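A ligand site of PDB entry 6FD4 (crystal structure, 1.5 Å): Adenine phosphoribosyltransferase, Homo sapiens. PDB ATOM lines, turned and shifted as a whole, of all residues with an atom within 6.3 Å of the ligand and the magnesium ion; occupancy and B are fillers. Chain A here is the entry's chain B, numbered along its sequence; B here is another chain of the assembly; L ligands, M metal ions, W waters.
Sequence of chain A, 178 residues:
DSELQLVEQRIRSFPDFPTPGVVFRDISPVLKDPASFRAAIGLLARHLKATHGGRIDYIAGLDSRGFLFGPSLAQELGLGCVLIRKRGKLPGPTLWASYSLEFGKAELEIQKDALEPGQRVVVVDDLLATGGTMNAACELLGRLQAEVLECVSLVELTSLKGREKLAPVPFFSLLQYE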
ATOM      1  N   LEU A  62      23.712  -3.378   8.136  1.00  0.00           N
ATOM      2  CA  LEU A  62      24.231  -1.996   8.236  1.00  0.00           C
ATOM      3  C   LEU A  62      23.227  -0.925   7.781  1.00  0.00           C
ATOM      4  O   LEU A  62      22.738  -0.911   6.646  1.00  0.00           O
ATOM      5  CB  LEU A  62      25.540  -1.873   7.437  1.00  0.00           C
ATOM      6  CG  LEU A  62      26.678  -2.821   7.831  1.00  0.00           C
ATOM      7  CD1 LEU A  62      27.985  -2.367   7.226  1.00  0.00           C
ATOM      8  CD2 LEU A  62      26.789  -3.001   9.325  1.00  0.00           C
ATOM      9  N   ASP A  63      22.911  -0.011   8.677  1.00  0.00           N
ATOM     10  CA  ASP A  63      22.076   1.157   8.398  1.00  0.00           C
ATOM     11  C   ASP A  63      22.638   1.947   7.205  1.00  0.00           C
ATOM     12  O   ASP A  63      23.834   2.220   7.211  1.00  0.00           O
ATOM     13  CB  ASP A  63      22.156   2.004   9.677  1.00  0.00           C
ATOM     14  CG  ASP A  63      21.221   3.194   9.713  1.00  0.00           C
ATOM     15  OD1 ASP A  63      20.491   3.484   8.738  1.00  0.00           O
ATOM     16  OD2 ASP A  63      21.221   3.850  10.792  1.00  0.00           O
ATOM     17  N   SER A  64      21.873   2.308   6.157  1.00  0.00           N
ATOM     18  CA  SER A  64      20.449   1.991   6.052  1.00  0.00           C
ATOM     19  C   SER A  64      20.153   0.951   4.977  1.00  0.00           C
ATOM     20  O   SER A  64      19.289   0.092   5.162  1.00  0.00           O
ATOM     21  CB  SER A  64      19.634   3.256   5.750  1.00  0.00           C
ATOM     22  OG  SER A  64      19.840   3.709   4.431  1.00  0.00           O
ATOM     23  N   ARG A  65      20.837   1.016   3.828  1.00  0.00           N
ATOM     24  CA  ARG A  65      20.500   0.056   2.765  1.00  0.00           C
ATOM     25  C   ARG A  65      20.730  -1.396   3.125  1.00  0.00           C
ATOM     26  O   ARG A  65      20.055  -2.302   2.592  1.00  0.00           O
ATOM     27  CB  ARG A  65      21.194   0.404   1.455  1.00  0.00           C
ATOM     28  CG  ARG A  65      20.564   1.600   0.786  1.00  0.00           C
ATOM     29  CD  ARG A  65      21.240   1.900  -0.541  1.00  0.00           C
ATOM     30  NE  ARG A  65      22.170   3.000  -0.365  1.00  0.00           N
ATOM     31  CZ  ARG A  65      23.229   3.279  -1.108  1.00  0.00           C
ATOM     32  NH1 ARG A  65      23.687   2.478  -2.046  1.00  0.00           N
ATOM     33  NH2 ARG A  65      23.887   4.384  -0.854  1.00  0.00           N
ATOM     34  N   GLY A  66      21.648  -1.671   4.034  1.00  0.00           N
ATOM     35  CA  GLY A  66      21.884  -3.035   4.478  1.00  0.00           C
ATOM     36  C   GLY A  66      20.714  -3.609   5.262  1.00  0.00           C
ATOM     37  O   GLY A  66      20.544  -4.816   5.347  1.00  0.00           O
ATOM     38  N   LYS A  86      23.794   4.298  12.035  1.00  0.00           N
ATOM     39  CA  LYS A  86      24.422   5.608  12.096  1.00  0.00           C
ATOM     40  C   LYS A  86      24.299   6.167  13.512  1.00  0.00           C
ATOM     41  O   LYS A  86      23.292   5.992  14.182  1.00  0.00           O
ATOM     42  CB  LYS A  86      23.793   6.536  11.069  1.00  0.00           C
ATOM     43  CG  LYS A  86      23.911   6.018   9.656  1.00  0.00           C
ATOM     44  CD  LYS A  86      25.342   6.021   9.164  1.00  0.00           C
ATOM     45  CE  LYS A  86      25.480   5.273   7.853  1.00  0.00           C
ATOM     46  NZ  LYS A  86      24.955   6.071   6.715  1.00  0.00           N
ATOM     47  N   TYR A  99      34.601   6.812  10.373  1.00  0.00           N
ATOM     48  CA  TYR A  99      35.186   6.410   9.124  1.00  0.00           C
ATOM     49  C   TYR A  99      34.935   7.552   8.142  1.00  0.00           C
ATOM     50  O   TYR A  99      34.127   8.438   8.417  1.00  0.00           O
ATOM     51  CB  TYR A  99      34.570   5.100   8.648  1.00  0.00           C
ATOM     52  CG  TYR A  99      33.083   5.166   8.382  1.00  0.00           C
ATOM     53  CD1 TYR A  99      32.168   5.220   9.417  1.00  0.00           C
ATOM     54  CD2 TYR A  99      32.591   5.167   7.072  1.00  0.00           C
ATOM     55  CE1 TYR A  99      30.804   5.298   9.172  1.00  0.00           C
ATOM     56  CE2 TYR A  99      31.213   5.220   6.820  1.00  0.00           C
ATOM     57  CZ  TYR A  99      30.341   5.288   7.875  1.00  0.00           C
ATOM     58  OH  TYR A  99      28.973   5.339   7.662  1.00  0.00           O
ATOM     59  N   SER A 100      35.664   7.555   7.032  1.00  0.00           N
ATOM     60  CA  SER A 100      35.616   8.643   6.070  1.00  0.00           C
ATOM     61  C   SER A 100      34.482   8.371   5.079  1.00  0.00           C
ATOM     62  O   SER A 100      34.446   7.299   4.474  1.00  0.00           O
ATOM     63  CB  SER A 100      36.942   8.710   5.338  1.00  0.00           C
ATOM     64  OG  SER A 100      36.974   9.734   4.365  1.00  0.00           O
ATOM     65  N   LEU A 101      33.555   9.314   4.952  1.00  0.00           N
ATOM     66  CA  LEU A 101      32.489   9.216   3.990  1.00  0.00           C
ATOM     67  C   LEU A 101      32.322  10.534   3.249  1.00  0.00           C
ATOM     68  O   LEU A 101      32.188  11.580   3.885  1.00  0.00           O
ATOM     69  CB  LEU A 101      31.182   8.855   4.710  1.00  0.00           C
ATOM     70  CG  LEU A 101      30.045   8.377   3.817  1.00  0.00           C
ATOM     71  CD1 LEU A 101      30.485   7.165   3.018  1.00  0.00           C
ATOM     72  CD2 LEU A 101      28.825   8.044   4.671  1.00  0.00           C
ATOM     73  N   ASP A 125      25.767  -5.788   3.800  1.00  0.00           N
ATOM     74  CA  ASP A 125      25.432  -4.447   3.318  1.00  0.00           C
ATOM     75  C   ASP A 125      25.062  -4.564   1.851  1.00  0.00           C
ATOM     76  O   ASP A 125      25.361  -5.589   1.205  1.00  0.00           O
ATOM     77  CB  ASP A 125      26.614  -3.500   3.499  1.00  0.00           C
ATOM     78  CG  ASP A 125      26.176  -2.048   3.655  1.00  0.00           C
ATOM     79  OD1 ASP A 125      24.950  -1.785   3.566  1.00  0.00           O
ATOM     80  OD2 ASP A 125      27.064  -1.196   3.876  1.00  0.00           O
ATOM     81  N   ASP A 126      24.439  -3.539   1.290  1.00  0.00           N
ATOM     82  CA  ASP A 126      24.078  -3.607  -0.096  1.00  0.00           C
ATOM     83  C   ASP A 126      25.310  -3.500  -1.010  1.00  0.00           C
ATOM     84  O   ASP A 126      25.375  -4.194  -2.023  1.00  0.00           O
ATOM     85  CB  ASP A 126      23.044  -2.538  -0.451  1.00  0.00           C
ATOM     86  CG  ASP A 126      23.597  -1.132  -0.441  1.00  0.00           C
ATOM     87  OD1 ASP A 126      24.293  -0.777   0.527  1.00  0.00           O
ATOM     88  OD2 ASP A 126      23.280  -0.365  -1.374  1.00  0.00           O
ATOM     89  N   LEU A 127      26.261  -2.654  -0.629  1.00  0.00           N
ATOM     90  CA  LEU A 127      27.339  -2.197  -1.538  1.00  0.00           C
ATOM     91  C   LEU A 127      28.645  -2.047  -0.778  1.00  0.00           C
ATOM     92  O   LEU A 127      28.672  -1.433   0.292  1.00  0.00           O
ATOM     93  CB  LEU A 127      26.979  -0.831  -2.126  1.00  0.00           C
ATOM     94  CG  LEU A 127      28.157  -0.065  -2.783  1.00  0.00           C
ATOM     95  CD1 LEU A 127      28.331  -0.597  -4.170  1.00  0.00           C
ATOM     96  CD2 LEU A 127      27.914   1.433  -2.841  1.00  0.00           C
ATOM     97  N   LEU A 128      29.723  -2.615  -1.319  1.00  0.00           N
ATOM     98  CA  LEU A 128      31.062  -2.355  -0.833  1.00  0.00           C
ATOM     99  C   LEU A 128      31.757  -1.443  -1.820  1.00  0.00           C
ATOM    100  O   LEU A 128      31.899  -1.775  -2.998  1.00  0.00           O
ATOM    101  CB  LEU A 128      31.867  -3.637  -0.695  1.00  0.00           C
ATOM    102  CG  LEU A 128      33.265  -3.467  -0.071  1.00  0.00           C
ATOM    103  CD1 LEU A 128      33.142  -3.394   1.436  1.00  0.00           C
ATOM    104  CD2 LEU A 128      34.175  -4.613  -0.460  1.00  0.00           C
ATOM    105  N   ALA A 129      32.196  -0.288  -1.335  1.00  0.00           N
ATOM    106  CA  ALA A 129      32.898   0.686  -2.187  1.00  0.00           C
ATOM    107  C   ALA A 129      34.300   0.855  -1.637  1.00  0.00           C
ATOM    108  O   ALA A 129      35.101  -0.044  -1.828  1.00  0.00           O
ATOM    109  CB  ALA A 129      32.137   1.982  -2.306  1.00  0.00           C
ATOM    110  N   THR A 130      34.612   1.949  -0.956  1.00  0.00           N
ATOM    111  CA  THR A 130      35.918   2.045  -0.291  1.00  0.00           C
ATOM    112  C   THR A 130      36.150   0.998   0.822  1.00  0.00           C
ATOM    113  O   THR A 130      37.292   0.733   1.200  1.00  0.00           O
ATOM    114  CB  THR A 130      36.170   3.436   0.329  1.00  0.00           C
ATOM    115  OG1 THR A 130      35.312   3.628   1.467  1.00  0.00           O
ATOM    116  CG2 THR A 130      35.945   4.517  -0.691  1.00  0.00           C
ATOM    117  N   GLY A 131      35.072   0.444   1.377  1.00  0.00           N
ATOM    118  CA  GLY A 131      35.175  -0.462   2.515  1.00  0.00           C
ATOM    119  C   GLY A 131      35.130   0.230   3.883  1.00  0.00           C
ATOM    120  O   GLY A 131      35.142  -0.429   4.926  1.00  0.00           O
ATOM    121  N   GLY A 132      35.019   1.555   3.892  1.00  0.00           N
ATOM    122  CA  GLY A 132      35.029   2.305   5.124  1.00  0.00           C
ATOM    123  C   GLY A 132      33.879   1.926   6.052  1.00  0.00           C
ATOM    124  O   GLY A 132      34.091   1.733   7.252  1.00  0.00           O
ATOM    125  N   THR A 133      32.677   1.780   5.504  1.00  0.00           N
ATOM    126  CA  THR A 133      31.502   1.470   6.306  1.00  0.00           C
ATOM    127  C   THR A 133      31.629   0.062   6.869  1.00  0.00           C
ATOM    128  O   THR A 133      31.427  -0.180   8.058  1.00  0.00           O
ATOM    129  CB  THR A 133      30.232   1.574   5.440  1.00  0.00           C
ATOM    130  OG1 THR A 133      30.143   2.867   4.886  1.00  0.00           O
ATOM    131  CG2 THR A 133      28.970   1.277   6.223  1.00  0.00           C
ATOM    132  N   MET A 134      31.960  -0.894   6.010  1.00  0.00           N
ATOM    133  CA  MET A 134      32.115  -2.277   6.453  1.00  0.00           C
ATOM    134  C   MET A 134      33.245  -2.441   7.465  1.00  0.00           C
ATOM    135  O   MET A 134      33.127  -3.214   8.415  1.00  0.00           O
ATOM    136  CB  MET A 134      32.346  -3.196   5.239  1.00  0.00           C
ATOM    137  CG  MET A 134      32.109  -4.658   5.530  1.00  0.00           C
ATOM    138  SD  MET A 134      30.377  -5.159   5.622  1.00  0.00           S
ATOM    139  CE  MET A 134      29.903  -5.253   3.902  1.00  0.00           C
ATOM    140  N   LEU A 160      37.940   0.261  -6.088  1.00  0.00           N
ATOM    141  CA  LEU A 160      38.123   0.992  -4.859  1.00  0.00           C
ATOM    142  C   LEU A 160      38.837   0.155  -3.779  1.00  0.00           C
ATOM    143  O   LEU A 160      39.181   0.665  -2.718  1.00  0.00           O
ATOM    144  CB  LEU A 160      36.783   1.528  -4.355  1.00  0.00           C
ATOM    145  CG  LEU A 160      36.057   2.514  -5.274  1.00  0.00           C
ATOM    146  CD1 LEU A 160      34.765   2.987  -4.630  1.00  0.00           C
ATOM    147  CD2 LEU A 160      36.931   3.709  -5.628  1.00  0.00           C
ATOM    148  N   ASP B  63      12.574   4.583   4.868  1.00  0.00           N
ATOM    149  CA  ASP B  63      13.940   4.764   5.376  1.00  0.00           C
ATOM    150  C   ASP B  63      13.892   5.352   6.784  1.00  0.00           C
ATOM    151  O   ASP B  63      13.192   6.355   6.973  1.00  0.00           O
ATOM    152  CB  ASP B  63      14.579   5.762   4.395  1.00  0.00           C
ATOM    153  CG  ASP B  63      16.042   6.007   4.592  1.00  0.00           C
ATOM    154  OD1 ASP B  63      16.671   5.448   5.514  1.00  0.00           O
ATOM    155  OD2 ASP B  63      16.571   6.772   3.767  1.00  0.00           O
ATOM    156  N   SER B  64      14.554   4.794   7.801  1.00  0.00           N
ATOM    157  CA  SER B  64      15.475   3.673   7.688  1.00  0.00           C
ATOM    158  C   SER B  64      14.911   2.418   8.355  1.00  0.00           C
ATOM    159  O   SER B  64      15.028   1.324   7.794  1.00  0.00           O
ATOM    160  CB  SER B  64      16.837   3.998   8.334  1.00  0.00           C
ATOM    161  OG  SER B  64      17.384   5.187   7.804  1.00  0.00           O
ATOM    162  N   ARG B  85      12.826   7.306   0.664  1.00  0.00           N
ATOM    163  CA  ARG B  85      14.106   7.562   1.361  1.00  0.00           C
ATOM    164  C   ARG B  85      14.177   8.941   1.944  1.00  0.00           C
ATOM    165  O   ARG B  85      13.444   9.840   1.541  1.00  0.00           O
ATOM    166  CB  ARG B  85      15.249   7.394   0.390  1.00  0.00           C
ATOM    167  CG  ARG B  85      15.481   5.952  -0.053  1.00  0.00           C
ATOM    168  CD  ARG B  85      16.951   5.587  -0.048  1.00  0.00           C
ATOM    169  NE  ARG B  85      17.517   5.696   1.297  1.00  0.00           N
ATOM    170  CZ  ARG B  85      18.798   5.512   1.612  1.00  0.00           C
ATOM    171  NH1 ARG B  85      19.673   5.139   0.693  1.00  0.00           N
ATOM    172  NH2 ARG B  85      19.203   5.712   2.856  1.00  0.00           N
ATOM    173  N   LYS B  89      19.380  10.744  -1.252  1.00  0.00           N
ATOM    174  CA  LYS B  89      19.942   9.408  -1.343  1.00  0.00           C
ATOM    175  C   LYS B  89      19.606   8.646  -2.618  1.00  0.00           C
ATOM    176  O   LYS B  89      20.233   7.627  -2.903  1.00  0.00           O
ATOM    177  CB  LYS B  89      19.489   8.595  -0.146  1.00  0.00           C
ATOM    178  CG  LYS B  89      19.845   9.239   1.193  1.00  0.00           C
ATOM    179  CD  LYS B  89      21.346   9.373   1.357  1.00  0.00           C
ATOM    180  CE  LYS B  89      22.057   8.037   1.291  1.00  0.00           C
ATOM    181  NZ  LYS B  89      23.537   8.232   1.328  1.00  0.00           N
HETATM  182  C1  LIG L   1      26.367   3.446   1.132  1.00  0.00           C
HETATM  183  C2  LIG L   1      26.080   1.963   0.993  1.00  0.00           C
HETATM  184  C3  LIG L   1      27.143   1.357   1.887  1.00  0.00           C
HETATM  185  C4  LIG L   1      28.304   2.347   1.827  1.00  0.00           C
HETATM  186  C5  LIG L   1      29.469   1.804   0.997  1.00  0.00           C
HETATM  187  O1  LIG L   1      25.790   3.896   2.360  1.00  0.00           O
HETATM  188  O2  LIG L   1      24.761   1.640   1.449  1.00  0.00           O
HETATM  189  O3  LIG L   1      26.676   1.272   3.260  1.00  0.00           O
HETATM  190  O4  LIG L   1      27.794   3.551   1.211  1.00  0.00           O
HETATM  191  O5  LIG L   1      30.488   2.816   0.839  1.00  0.00           O
HETATM  192  P1  LIG L   1      31.957   2.576   1.424  1.00  0.00           P
HETATM  193  O6  LIG L   1      32.329   1.144   1.162  1.00  0.00           O
HETATM  194  O7  LIG L   1      31.879   2.861   2.925  1.00  0.00           O
HETATM  195  O8  LIG L   1      32.809   3.546   0.637  1.00  0.00           O
HETATM  196  P2  LIG L   1      25.510   5.455   2.664  1.00  0.00           P
HETATM  197  O9  LIG L   1      26.462   5.872   3.745  1.00  0.00           O
HETATM  198  O10 LIG L   1      25.561   6.190   1.370  1.00  0.00           O
HETATM  199  O11 LIG L   1      24.076   5.455   3.383  1.00  0.00           O
HETATM  200  P3  LIG L   1      22.706   4.659   3.140  1.00  0.00           P
HETATM  201  O12 LIG L   1      22.978   3.238   3.635  1.00  0.00           O
HETATM  202  O13 LIG L   1      21.760   5.407   4.034  1.00  0.00           O
HETATM  203  O14 LIG L   1      22.362   4.746   1.671  1.00  0.00           O
HETATM  204 MG    MG M   1      24.762   2.244   3.598  1.00  0.00          MG
HETATM  205  O   HOH W   1      27.880   4.309   5.404  1.00  0.00           O
HETATM  206  O   HOH W   2      31.973  -0.586   3.220  1.00  0.00           O
HETATM  207  O   HOH W   3      33.328   4.973   3.862  1.00  0.00           O
HETATM  208  O   HOH W   4      22.237   5.794   6.636  1.00  0.00           O
HETATM  209  O   HOH W   5      29.222   5.155  -0.242  1.00  0.00           O
HETATM  210  O   HOH W   6      31.843   5.787  -0.377  1.00  0.00           O
HETATM  211  O   HOH W   7      23.985   0.406   4.407  1.00  0.00           O
HETATM  212  O   HOH W   8      25.460   3.046   5.247  1.00  0.00           O
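Water W8 lies within hydrogen-bond range of O of Asp 63 of chain A (2.7 Å), O11 of the ligand (3.3 Å) and NZ of Lys 86 (3.4 Å).
Water W4 bridges O13 of the ligand and NZ of Lys 86.
Water W1 lies within hydrogen-bond range of an oxygen (O9) of the ligand, the side-chain hydroxyl of Tyr 99 and the side-chain hydroxyl of Thr 133.
Water W2 lies within hydrogen-bond range of an oxygen (O6) of the ligand (2.7 Å), the backbone NH (N) of Met 134 (2.8 Å) and the backbone NH (N) of Thr 133 (3.4 Å).
Water W3 lies within hydrogen-bond range of the backbone carbonyl oxygen of Ser 100, an oxygen (O7) of the ligand and the side-chain hydroxyl of Thr 130.
Merely in contact with the magnesium ion: Asp 63 of chain A and Ser 64 of chain A.
Of the 24 residues printed, 2 come within 4 Å of the magnesium ion.
N of Gly 66 sits at hydrogen-bond distance from OD1 of Asp 125, at 3.3 Å.
The side-chain hydroxyl (OG1) of Thr 130 lies within hydrogen-bond range of the backbone NH (N) of Gly 132.
The side-chain carboxylate (OD2) of Asp 126 is in salt-bridge range of the guanidinium group (NH1) of Arg 65 (2.9 Å).
N of Lys 86 lies within hydrogen-bond range of OD2 of Asp 63 of chain A, 2.9 Å away.
The guanidinium group (NE) of Arg 85 of chain B lies within salt-bridge range of the side-chain carboxylate (OD2) of Asp 63 of chain B (2.9 Å).
The side-chain hydroxyl of Ser 64 of chain A lies within hydrogen-bond range of the guanidinium group of Arg 85 of chain B, at 2.6 Å.
O12 of the ligand sits close to N of Arg 65, at 3.1 Å.
O7 of the ligand lies within hydrogen-bond range of OG1 of Thr 133 (2.6 Å).
N of Ser 64 of chain A sits close to O12 of the ligand, at 2.9 Å.
The guanidinium group (NH2) of Arg 85 of chain B is in salt-bridge range of an oxygen (O13) of the ligand.
N of Gly 131 sits at hydrogen-bond distance from O6 of the ligand (2.8 Å).
An oxygen (O2) of the ligand lies close to the side-chain carboxylate of Asp 126 (2.6 Å).
The side-chain amino group (NZ) of Lys 89 of chain B lies within salt-bridge range of an oxygen (O10) of the ligand, at 2.9 Å.
The backbone NH of Thr 133 lies within hydrogen-bond range of an oxygen (O7) of the ligand.
O8 of the ligand is in hydrogen-bond range of OG1 of Thr 130 (2.6 Å).
An oxygen (O3) of the ligand sits close to the side-chain carboxylate (OD2) of Asp 125.
An oxygen (O8) of the ligand sits at hydrogen-bond distance from the backbone NH (N) of Thr 130 (2.9 Å).
The backbone NH (N) of Ala 129 sits at hydrogen-bond distance from an oxygen (O6) of the ligand (2.9 Å).
The guanidinium group (NE) of Arg 65 is in salt-bridge range of an oxygen (O14) of the ligand.
NZ of Lys 86 lies within salt-bridge range of O9 of the ligand, at 3.3 Å.
OG of Ser 64 of chain A lies within hydrogen-bond range of O13 of the ligand, at 2.6 Å.
The magnesium ion is bound by water W8 (2.0 Å), O12 of the ligand (2.0 Å), water W7 (2.2 Å), O3 of the ligand (2.2 Å), O2 of the ligand (2.2 Å) and O1 of the ligand (2.3 Å).
Residues that only touch the ligand: Asp 63 of chain A, Leu 101, Leu 127, Leu 128 and Gly 132.
Hydrophobic or aromatic side chains that line the ligand: Leu 101 and Ala 129.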
